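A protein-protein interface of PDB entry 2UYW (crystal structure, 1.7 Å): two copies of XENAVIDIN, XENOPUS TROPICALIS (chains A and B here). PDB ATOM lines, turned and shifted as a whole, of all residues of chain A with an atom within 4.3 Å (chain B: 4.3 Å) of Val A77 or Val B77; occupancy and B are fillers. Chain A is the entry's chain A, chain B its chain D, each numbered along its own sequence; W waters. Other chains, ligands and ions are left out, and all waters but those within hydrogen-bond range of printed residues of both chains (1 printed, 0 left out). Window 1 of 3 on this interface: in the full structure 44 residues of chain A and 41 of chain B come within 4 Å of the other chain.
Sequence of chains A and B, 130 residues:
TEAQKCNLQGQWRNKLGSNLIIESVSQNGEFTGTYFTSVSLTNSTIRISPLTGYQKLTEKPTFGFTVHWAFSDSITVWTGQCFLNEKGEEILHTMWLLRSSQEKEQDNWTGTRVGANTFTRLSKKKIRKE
Gly A64 touches Thr B66, and with the chains exchanged Thr A66 touches Gly B64.
Gly A64 touches Val B77, and with the chains exchanged Val A77 touches Gly B64.
Phe A65 touches Thr B66, and with the chains exchanged Thr A66 touches Phe B65.
Trp A96 touches Leu B97, and with the chains exchanged Leu A97 touches Trp B96.
10 positions are printed for both chains.
Of the 17 pairs that touch across the chains among the printed residues, 16 have their exchanged pair printed and touching as well.
The side-chain hydroxyl (OG1) of Thr A66 is in hydrogen-bond range of the backbone NH (N) of Phe B65, at 3.5 Å.
N of Phe A65 is in hydrogen-bond range of OG1 of Thr B66 (3.5 Å).
Printed residues of chain B within 4 Å of Gly A64: Thr B66 (3.5 Å) and Val B77 (3.97 Å).
Thr A76 touches none of the printed residues of chain B.
Val A77 touches just these residues of chain B: Gly B64 (3.9 Å), Val B77 (3.5 Å) and Trp B78 (3.5 Å).
Of the printed residues of chain B, Met A95 touches Leu B97 (3.5 Å).
Printed residues of chain A within 4 Å of Gly B64: Thr A66 (3.4 Å) and Val A77 (3.9 Å).
Of the printed residues of chain A, Thr B66 touches Gly A64 (3.5 Å) and Phe A65 (3.5 Å).
Thr B76 touches none of the printed residues of chain A.
Of the printed residues of chain A, Val B77 touches Gly A64 (3.97 Å), Val A77 (3.5 Å), Trp A78 (3.5 Å) and Thr A79 (3.98 Å).
Printed residues of chain A within 4 Å of Met B95: Leu A97 (3.6 Å).
The nearest residue of chain B that does not touch Val A77 is Thr B79 (4.04 Å).
The nearest printed residue of chain A that does not touch Leu B97 is Val A77 (4.9 Å).
Gly A64 touches Thr B66.
Gly B64 touches Thr A66.
CG2 of Val A77 touches CG2 of Val B77, 3.5 Å away.
Val B77 touches Trp A78.
Thr A79 touches Leu B97.
Leu B97 touches Met A95 (CD1 to O, 3.5 Å).
Leu A97 touches Thr B79.
CD1 of Leu A97 touches O of Met B95, 3.6 Å away.
N of Trp B96 touches CD1 of Leu A97, 3.9 Å away.
Leu B97 touches Leu A97.
Water W1 bridges the side-chain hydroxyl of Thr B66 (2.8 Å) and the side-chain hydroxyl of Thr A66 (2.8 Å).
Printed residues of chain A that touch a printed residue of chain B: Gly A64, Phe A65, Thr A66, Val A77, Trp A78, Thr A79, Met A95, Trp A96 and Leu A97.
Of the 10 printed residues of chain B, 9 touch a printed residue of chain A.
Hydrophobic or aromatic side chains of chain B within 4 Å of the printed part of chain A: Val B77, Met B95 and Leu B97.
Among the printed residues, 17 pairs touch across the chains.
The backbone carbonyl oxygen (O) of Met A95 sits at hydrogen-bond distance from the backbone NH (N) of Thr A79, 2.9 Å away.
The backbone NH (N) of Phe B65 sits at hydrogen-bond distance from the backbone carbonyl oxygen (O) of Trp B78.
N of Val B77 lies within hydrogen-bond range of O of Leu B97 (2.9 Å).
The backbone NH of Thr B79 lies within hydrogen-bond range of the backbone carbonyl oxygen of Met B95.
The backbone NH (N) of Val A77 is in hydrogen-bond range of the backbone carbonyl oxygen (O) of Leu A97, at 2.9 Å.
The backbone NH (N) of Trp A78 lies within hydrogen-bond range of the backbone carbonyl oxygen (O) of Phe A65 (2.9 Å).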
ATOM      1  N   GLY A  64      31.106 -29.858 -17.490  1.00  0.00           N
ATOM      2  CA  GLY A  64      30.335 -29.152 -18.516  1.00  0.00           C
ATOM      3  C   GLY A  64      29.149 -28.514 -17.825  1.00  0.00           C
ATOM      4  O   GLY A  64      28.702 -28.985 -16.761  1.00  0.00           O
ATOM      5  N   PHE A  65      28.644 -27.432 -18.411  1.00  0.00           N
ATOM      6  CA  PHE A  65      27.422 -26.829 -17.905  1.00  0.00           C
ATOM      7  C   PHE A  65      26.731 -25.977 -18.967  1.00  0.00           C
ATOM      8  O   PHE A  65      27.345 -25.598 -19.973  1.00  0.00           O
ATOM      9  CB  PHE A  65      27.674 -25.991 -16.639  1.00  0.00           C
ATOM     10  CG  PHE A  65      28.657 -24.848 -16.825  1.00  0.00           C
ATOM     11  CD1 PHE A  65      28.215 -23.582 -17.193  1.00  0.00           C
ATOM     12  CD2 PHE A  65      30.015 -25.043 -16.567  1.00  0.00           C
ATOM     13  CE1 PHE A  65      29.145 -22.501 -17.329  1.00  0.00           C
ATOM     14  CE2 PHE A  65      30.937 -23.999 -16.707  1.00  0.00           C
ATOM     15  CZ  PHE A  65      30.502 -22.722 -17.090  1.00  0.00           C
ATOM     16  N   THR A  66      25.462 -25.702 -18.707  1.00  0.00           N
ATOM     17  CA  THR A  66      24.625 -24.875 -19.580  1.00  0.00           C
ATOM     18  C   THR A  66      24.181 -23.635 -18.809  1.00  0.00           C
ATOM     19  O   THR A  66      23.719 -23.767 -17.631  1.00  0.00           O
ATOM     20  CB  THR A  66      23.325 -25.665 -19.958  1.00  0.00           C
ATOM     21  OG1 THR A  66      23.666 -26.889 -20.614  1.00  0.00           O
ATOM     22  CG2 THR A  66      22.413 -24.859 -20.914  1.00  0.00           C
ATOM     23  N   THR A  76      24.137 -20.862 -23.826  1.00  0.00           N
ATOM     24  CA  THR A  76      25.552 -21.226 -23.985  1.00  0.00           C
ATOM     25  C   THR A  76      25.867 -22.460 -23.187  1.00  0.00           C
ATOM     26  O   THR A  76      25.359 -22.629 -22.061  1.00  0.00           O
ATOM     27  CB  THR A  76      26.468 -20.076 -23.567  1.00  0.00           C
ATOM     28  OG1 THR A  76      26.115 -18.900 -24.316  1.00  0.00           O
ATOM     29  CG2 THR A  76      27.958 -20.416 -23.831  1.00  0.00           C
ATOM     30  N   VAL A  77      26.683 -23.329 -23.783  1.00  0.00           N
ATOM     31  CA  VAL A  77      27.259 -24.471 -23.039  1.00  0.00           C
ATOM     32  C   VAL A  77      28.775 -24.345 -22.989  1.00  0.00           C
ATOM     33  O   VAL A  77      29.398 -23.865 -23.955  1.00  0.00           O
ATOM     34  CB  VAL A  77      26.840 -25.839 -23.651  1.00  0.00           C
ATOM     35  CG1 VAL A  77      25.289 -26.064 -23.528  1.00  0.00           C
ATOM     36  CG2 VAL A  77      27.276 -25.953 -25.133  1.00  0.00           C
ATOM     37  N   TRP A  78      29.382 -24.734 -21.869  1.00  0.00           N
ATOM     38  CA  TRP A  78      30.852 -24.816 -21.757  1.00  0.00           C
ATOM     39  C   TRP A  78      31.234 -26.243 -21.423  1.00  0.00           C
ATOM     40  O   TRP A  78      30.510 -26.937 -20.683  1.00  0.00           O
ATOM     41  CB  TRP A  78      31.347 -23.965 -20.581  1.00  0.00           C
ATOM     42  CG  TRP A  78      31.403 -22.489 -20.765  1.00  0.00           C
ATOM     43  CD1 TRP A  78      32.519 -21.725 -20.978  1.00  0.00           C
ATOM     44  CD2 TRP A  78      30.299 -21.586 -20.690  1.00  0.00           C
ATOM     45  NE1 TRP A  78      32.166 -20.391 -21.061  1.00  0.00           N
ATOM     46  CE2 TRP A  78      30.813 -20.280 -20.862  1.00  0.00           C
ATOM     47  CE3 TRP A  78      28.918 -21.755 -20.467  1.00  0.00           C
ATOM     48  CZ2 TRP A  78      29.991 -19.141 -20.830  1.00  0.00           C
ATOM     49  CZ3 TRP A  78      28.103 -20.631 -20.435  1.00  0.00           C
ATOM     50  CH2 TRP A  78      28.636 -19.343 -20.617  1.00  0.00           C
ATOM     51  N   THR A  79      32.394 -26.682 -21.921  1.00  0.00           N
ATOM     52  CA  THR A  79      32.985 -27.894 -21.351  1.00  0.00           C
ATOM     53  C   THR A  79      34.473 -27.678 -21.226  1.00  0.00           C
ATOM     54  O   THR A  79      35.083 -26.979 -22.055  1.00  0.00           O
ATOM     55  CB  THR A  79      32.632 -29.171 -22.199  1.00  0.00           C
ATOM     56  OG1 THR A  79      33.041 -30.354 -21.499  1.00  0.00           O
ATOM     57  CG2 THR A  79      33.248 -29.129 -23.615  1.00  0.00           C
ATOM     58  N   MET A  95      36.010 -24.588 -23.589  1.00  0.00           N
ATOM     59  CA  MET A  95      35.504 -24.186 -24.890  1.00  0.00           C
ATOM     60  C   MET A  95      33.994 -24.056 -24.728  1.00  0.00           C
ATOM     61  O   MET A  95      33.390 -24.780 -23.912  1.00  0.00           O
ATOM     62  CB  MET A  95      35.825 -25.232 -25.958  1.00  0.00           C
ATOM     63  CG  MET A  95      37.308 -25.447 -26.196  1.00  0.00           C
ATOM     64  SD  MET A  95      38.044 -24.039 -27.051  1.00  0.00           S
ATOM     65  CE  MET A  95      37.245 -24.009 -28.627  1.00  0.00           C
ATOM     66  N   TRP A  96      33.374 -23.181 -25.514  1.00  0.00           N
ATOM     67  CA  TRP A  96      31.937 -22.907 -25.388  1.00  0.00           C
ATOM     68  C   TRP A  96      31.282 -22.857 -26.778  1.00  0.00           C
ATOM     69  O   TRP A  96      31.960 -22.567 -27.792  1.00  0.00           O
ATOM     70  CB  TRP A  96      31.656 -21.601 -24.599  1.00  0.00           C
ATOM     71  CG  TRP A  96      32.351 -20.315 -25.079  1.00  0.00           C
ATOM     72  CD1 TRP A  96      33.465 -19.711 -24.531  1.00  0.00           C
ATOM     73  CD2 TRP A  96      31.924 -19.456 -26.154  1.00  0.00           C
ATOM     74  NE1 TRP A  96      33.776 -18.556 -25.229  1.00  0.00           N
ATOM     75  CE2 TRP A  96      32.845 -18.368 -26.213  1.00  0.00           C
ATOM     76  CE3 TRP A  96      30.879 -19.515 -27.090  1.00  0.00           C
ATOM     77  CZ2 TRP A  96      32.744 -17.335 -27.166  1.00  0.00           C
ATOM     78  CZ3 TRP A  96      30.778 -18.473 -28.056  1.00  0.00           C
ATOM     79  CH2 TRP A  96      31.698 -17.397 -28.066  1.00  0.00           C
ATOM     80  N   LEU A  97      29.999 -23.161 -26.793  1.00  0.00           N
ATOM     81  CA  LEU A  97      29.095 -22.974 -27.952  1.00  0.00           C
ATOM     82  C   LEU A  97      27.966 -22.059 -27.491  1.00  0.00           C
ATOM     83  O   LEU A  97      27.315 -22.327 -26.465  1.00  0.00           O
ATOM     84  CB  LEU A  97      28.486 -24.317 -28.393  1.00  0.00           C
ATOM     85  CG  LEU A  97      29.510 -25.309 -28.940  1.00  0.00           C
ATOM     86  CD1 LEU A  97      28.793 -26.616 -29.178  1.00  0.00           C
ATOM     87  CD2 LEU A  97      30.186 -24.783 -30.271  1.00  0.00           C
ATOM     88  N   GLY B  64      20.178 -26.399 -24.331  1.00  0.00           N
ATOM     89  CA  GLY B  64      21.544 -26.929 -24.155  1.00  0.00           C
ATOM     90  C   GLY B  64      21.493 -27.963 -23.045  1.00  0.00           C
ATOM     91  O   GLY B  64      20.655 -27.862 -22.129  1.00  0.00           O
ATOM     92  N   PHE B  65      22.379 -28.947 -23.104  1.00  0.00           N
ATOM     93  CA  PHE B  65      22.481 -29.919 -21.995  1.00  0.00           C
ATOM     94  C   PHE B  65      23.869 -30.512 -21.921  1.00  0.00           C
ATOM     95  O   PHE B  65      24.620 -30.480 -22.900  1.00  0.00           O
ATOM     96  CB  PHE B  65      21.417 -31.039 -22.089  1.00  0.00           C
ATOM     97  CG  PHE B  65      21.485 -31.880 -23.359  1.00  0.00           C
ATOM     98  CD1 PHE B  65      22.214 -33.066 -23.396  1.00  0.00           C
ATOM     99  CD2 PHE B  65      20.735 -31.506 -24.483  1.00  0.00           C
ATOM    100  CE1 PHE B  65      22.240 -33.842 -24.579  1.00  0.00           C
ATOM    101  CE2 PHE B  65      20.766 -32.253 -25.678  1.00  0.00           C
ATOM    102  CZ  PHE B  65      21.536 -33.429 -25.715  1.00  0.00           C
ATOM    103  N   THR B  66      24.164 -31.104 -20.773  1.00  0.00           N
ATOM    104  CA  THR B  66      25.447 -31.797 -20.530  1.00  0.00           C
ATOM    105  C   THR B  66      25.166 -33.256 -20.236  1.00  0.00           C
ATOM    106  O   THR B  66      24.239 -33.560 -19.452  1.00  0.00           O
ATOM    107  CB  THR B  66      26.144 -31.197 -19.283  1.00  0.00           C
ATOM    108  OG1 THR B  66      26.303 -29.785 -19.425  1.00  0.00           O
ATOM    109  CG2 THR B  66      27.501 -31.846 -19.027  1.00  0.00           C
ATOM    110  N   THR B  76      30.258 -34.408 -22.499  1.00  0.00           N
ATOM    111  CA  THR B  76      29.835 -33.776 -23.766  1.00  0.00           C
ATOM    112  C   THR B  76      28.732 -32.772 -23.463  1.00  0.00           C
ATOM    113  O   THR B  76      27.895 -33.028 -22.589  1.00  0.00           O
ATOM    114  CB  THR B  76      29.330 -34.807 -24.814  1.00  0.00           C
ATOM    115  OG1 THR B  76      30.354 -35.785 -25.070  1.00  0.00           O
ATOM    116  CG2 THR B  76      28.934 -34.084 -26.136  1.00  0.00           C
ATOM    117  N   VAL B  77      28.773 -31.641 -24.177  1.00  0.00           N
ATOM    118  CA  VAL B  77      27.682 -30.659 -24.143  1.00  0.00           C
ATOM    119  C   VAL B  77      27.110 -30.522 -25.550  1.00  0.00           C
ATOM    120  O   VAL B  77      27.867 -30.628 -26.530  1.00  0.00           O
ATOM    121  CB  VAL B  77      28.137 -29.291 -23.546  1.00  0.00           C
ATOM    122  CG1 VAL B  77      28.510 -29.441 -22.034  1.00  0.00           C
ATOM    123  CG2 VAL B  77      29.318 -28.674 -24.355  1.00  0.00           C
ATOM    124  N   TRP B  78      25.788 -30.331 -25.633  1.00  0.00           N
ATOM    125  CA  TRP B  78      25.116 -30.006 -26.890  1.00  0.00           C
ATOM    126  C   TRP B  78      24.353 -28.715 -26.729  1.00  0.00           C
ATOM    127  O   TRP B  78      23.803 -28.433 -25.649  1.00  0.00           O
ATOM    128  CB  TRP B  78      24.045 -31.047 -27.228  1.00  0.00           C
ATOM    129  CG  TRP B  78      24.526 -32.404 -27.750  1.00  0.00           C
ATOM    130  CD1 TRP B  78      24.443 -32.841 -29.028  1.00  0.00           C
ATOM    131  CD2 TRP B  78      25.031 -33.484 -26.974  1.00  0.00           C
ATOM    132  NE1 TRP B  78      24.874 -34.156 -29.107  1.00  0.00           N
ATOM    133  CE2 TRP B  78      25.265 -34.561 -27.862  1.00  0.00           C
ATOM    134  CE3 TRP B  78      25.311 -33.650 -25.593  1.00  0.00           C
ATOM    135  CZ2 TRP B  78      25.750 -35.813 -27.427  1.00  0.00           C
ATOM    136  CZ3 TRP B  78      25.814 -34.889 -25.149  1.00  0.00           C
ATOM    137  CH2 TRP B  78      26.035 -35.955 -26.078  1.00  0.00           C
ATOM    138  N   THR B  79      24.283 -27.953 -27.809  1.00  0.00           N
ATOM    139  CA  THR B  79      23.338 -26.839 -27.853  1.00  0.00           C
ATOM    140  C   THR B  79      22.680 -26.780 -29.228  1.00  0.00           C
ATOM    141  O   THR B  79      23.310 -27.064 -30.259  1.00  0.00           O
ATOM    142  CB  THR B  79      23.951 -25.488 -27.381  1.00  0.00           C
ATOM    143  OG1 THR B  79      22.904 -24.521 -27.263  1.00  0.00           O
ATOM    144  CG2 THR B  79      24.973 -24.947 -28.388  1.00  0.00           C
ATOM    145  N   MET B  95      24.867 -28.638 -32.199  1.00  0.00           N
ATOM    146  CA  MET B  95      26.323 -28.778 -32.230  1.00  0.00           C
ATOM    147  C   MET B  95      26.762 -29.259 -30.866  1.00  0.00           C
ATOM    148  O   MET B  95      26.127 -28.935 -29.841  1.00  0.00           O
ATOM    149  CB  MET B  95      26.994 -27.427 -32.517  1.00  0.00           C
ATOM    150  CG  MET B  95      26.656 -26.873 -33.930  1.00  0.00           C
ATOM    151  SD  MET B  95      27.432 -27.827 -35.282  1.00  0.00           S
ATOM    152  CE  MET B  95      29.151 -27.757 -34.999  1.00  0.00           C
ATOM    153  N   TRP B  96      27.881 -29.984 -30.839  1.00  0.00           N
ATOM    154  CA  TRP B  96      28.400 -30.526 -29.584  1.00  0.00           C
ATOM    155  C   TRP B  96      29.900 -30.316 -29.423  1.00  0.00           C
ATOM    156  O   TRP B  96      30.613 -30.160 -30.419  1.00  0.00           O
ATOM    157  CB  TRP B  96      28.043 -32.039 -29.426  1.00  0.00           C
ATOM    158  CG  TRP B  96      28.463 -32.966 -30.600  1.00  0.00           C
ATOM    159  CD1 TRP B  96      27.673 -33.410 -31.640  1.00  0.00           C
ATOM    160  CD2 TRP B  96      29.771 -33.524 -30.826  1.00  0.00           C
ATOM    161  NE1 TRP B  96      28.421 -34.225 -32.498  1.00  0.00           N
ATOM    162  CE2 TRP B  96      29.694 -34.327 -32.003  1.00  0.00           C
ATOM    163  CE3 TRP B  96      30.987 -33.476 -30.118  1.00  0.00           C
ATOM    164  CZ2 TRP B  96      30.798 -35.041 -32.506  1.00  0.00           C
ATOM    165  CZ3 TRP B  96      32.101 -34.186 -30.637  1.00  0.00           C
ATOM    166  CH2 TRP B  96      31.978 -34.974 -31.812  1.00  0.00           C
ATOM    167  N   LEU B  97      30.340 -30.312 -28.153  1.00  0.00           N
ATOM    168  CA  LEU B  97      31.757 -30.333 -27.756  1.00  0.00           C
ATOM    169  C   LEU B  97      31.925 -31.540 -26.835  1.00  0.00           C
ATOM    170  O   LEU B  97      31.187 -31.672 -25.847  1.00  0.00           O
ATOM    171  CB  LEU B  97      32.146 -29.055 -26.968  1.00  0.00           C
ATOM    172  CG  LEU B  97      32.105 -27.730 -27.744  1.00  0.00           C
ATOM    173  CD1 LEU B  97      32.336 -26.524 -26.784  1.00  0.00           C
ATOM    174  CD2 LEU B  97      33.093 -27.713 -28.946  1.00  0.00           C
HETATM  175  O   HOH W   1      23.931 -28.734 -18.461  1.00  0.00           O
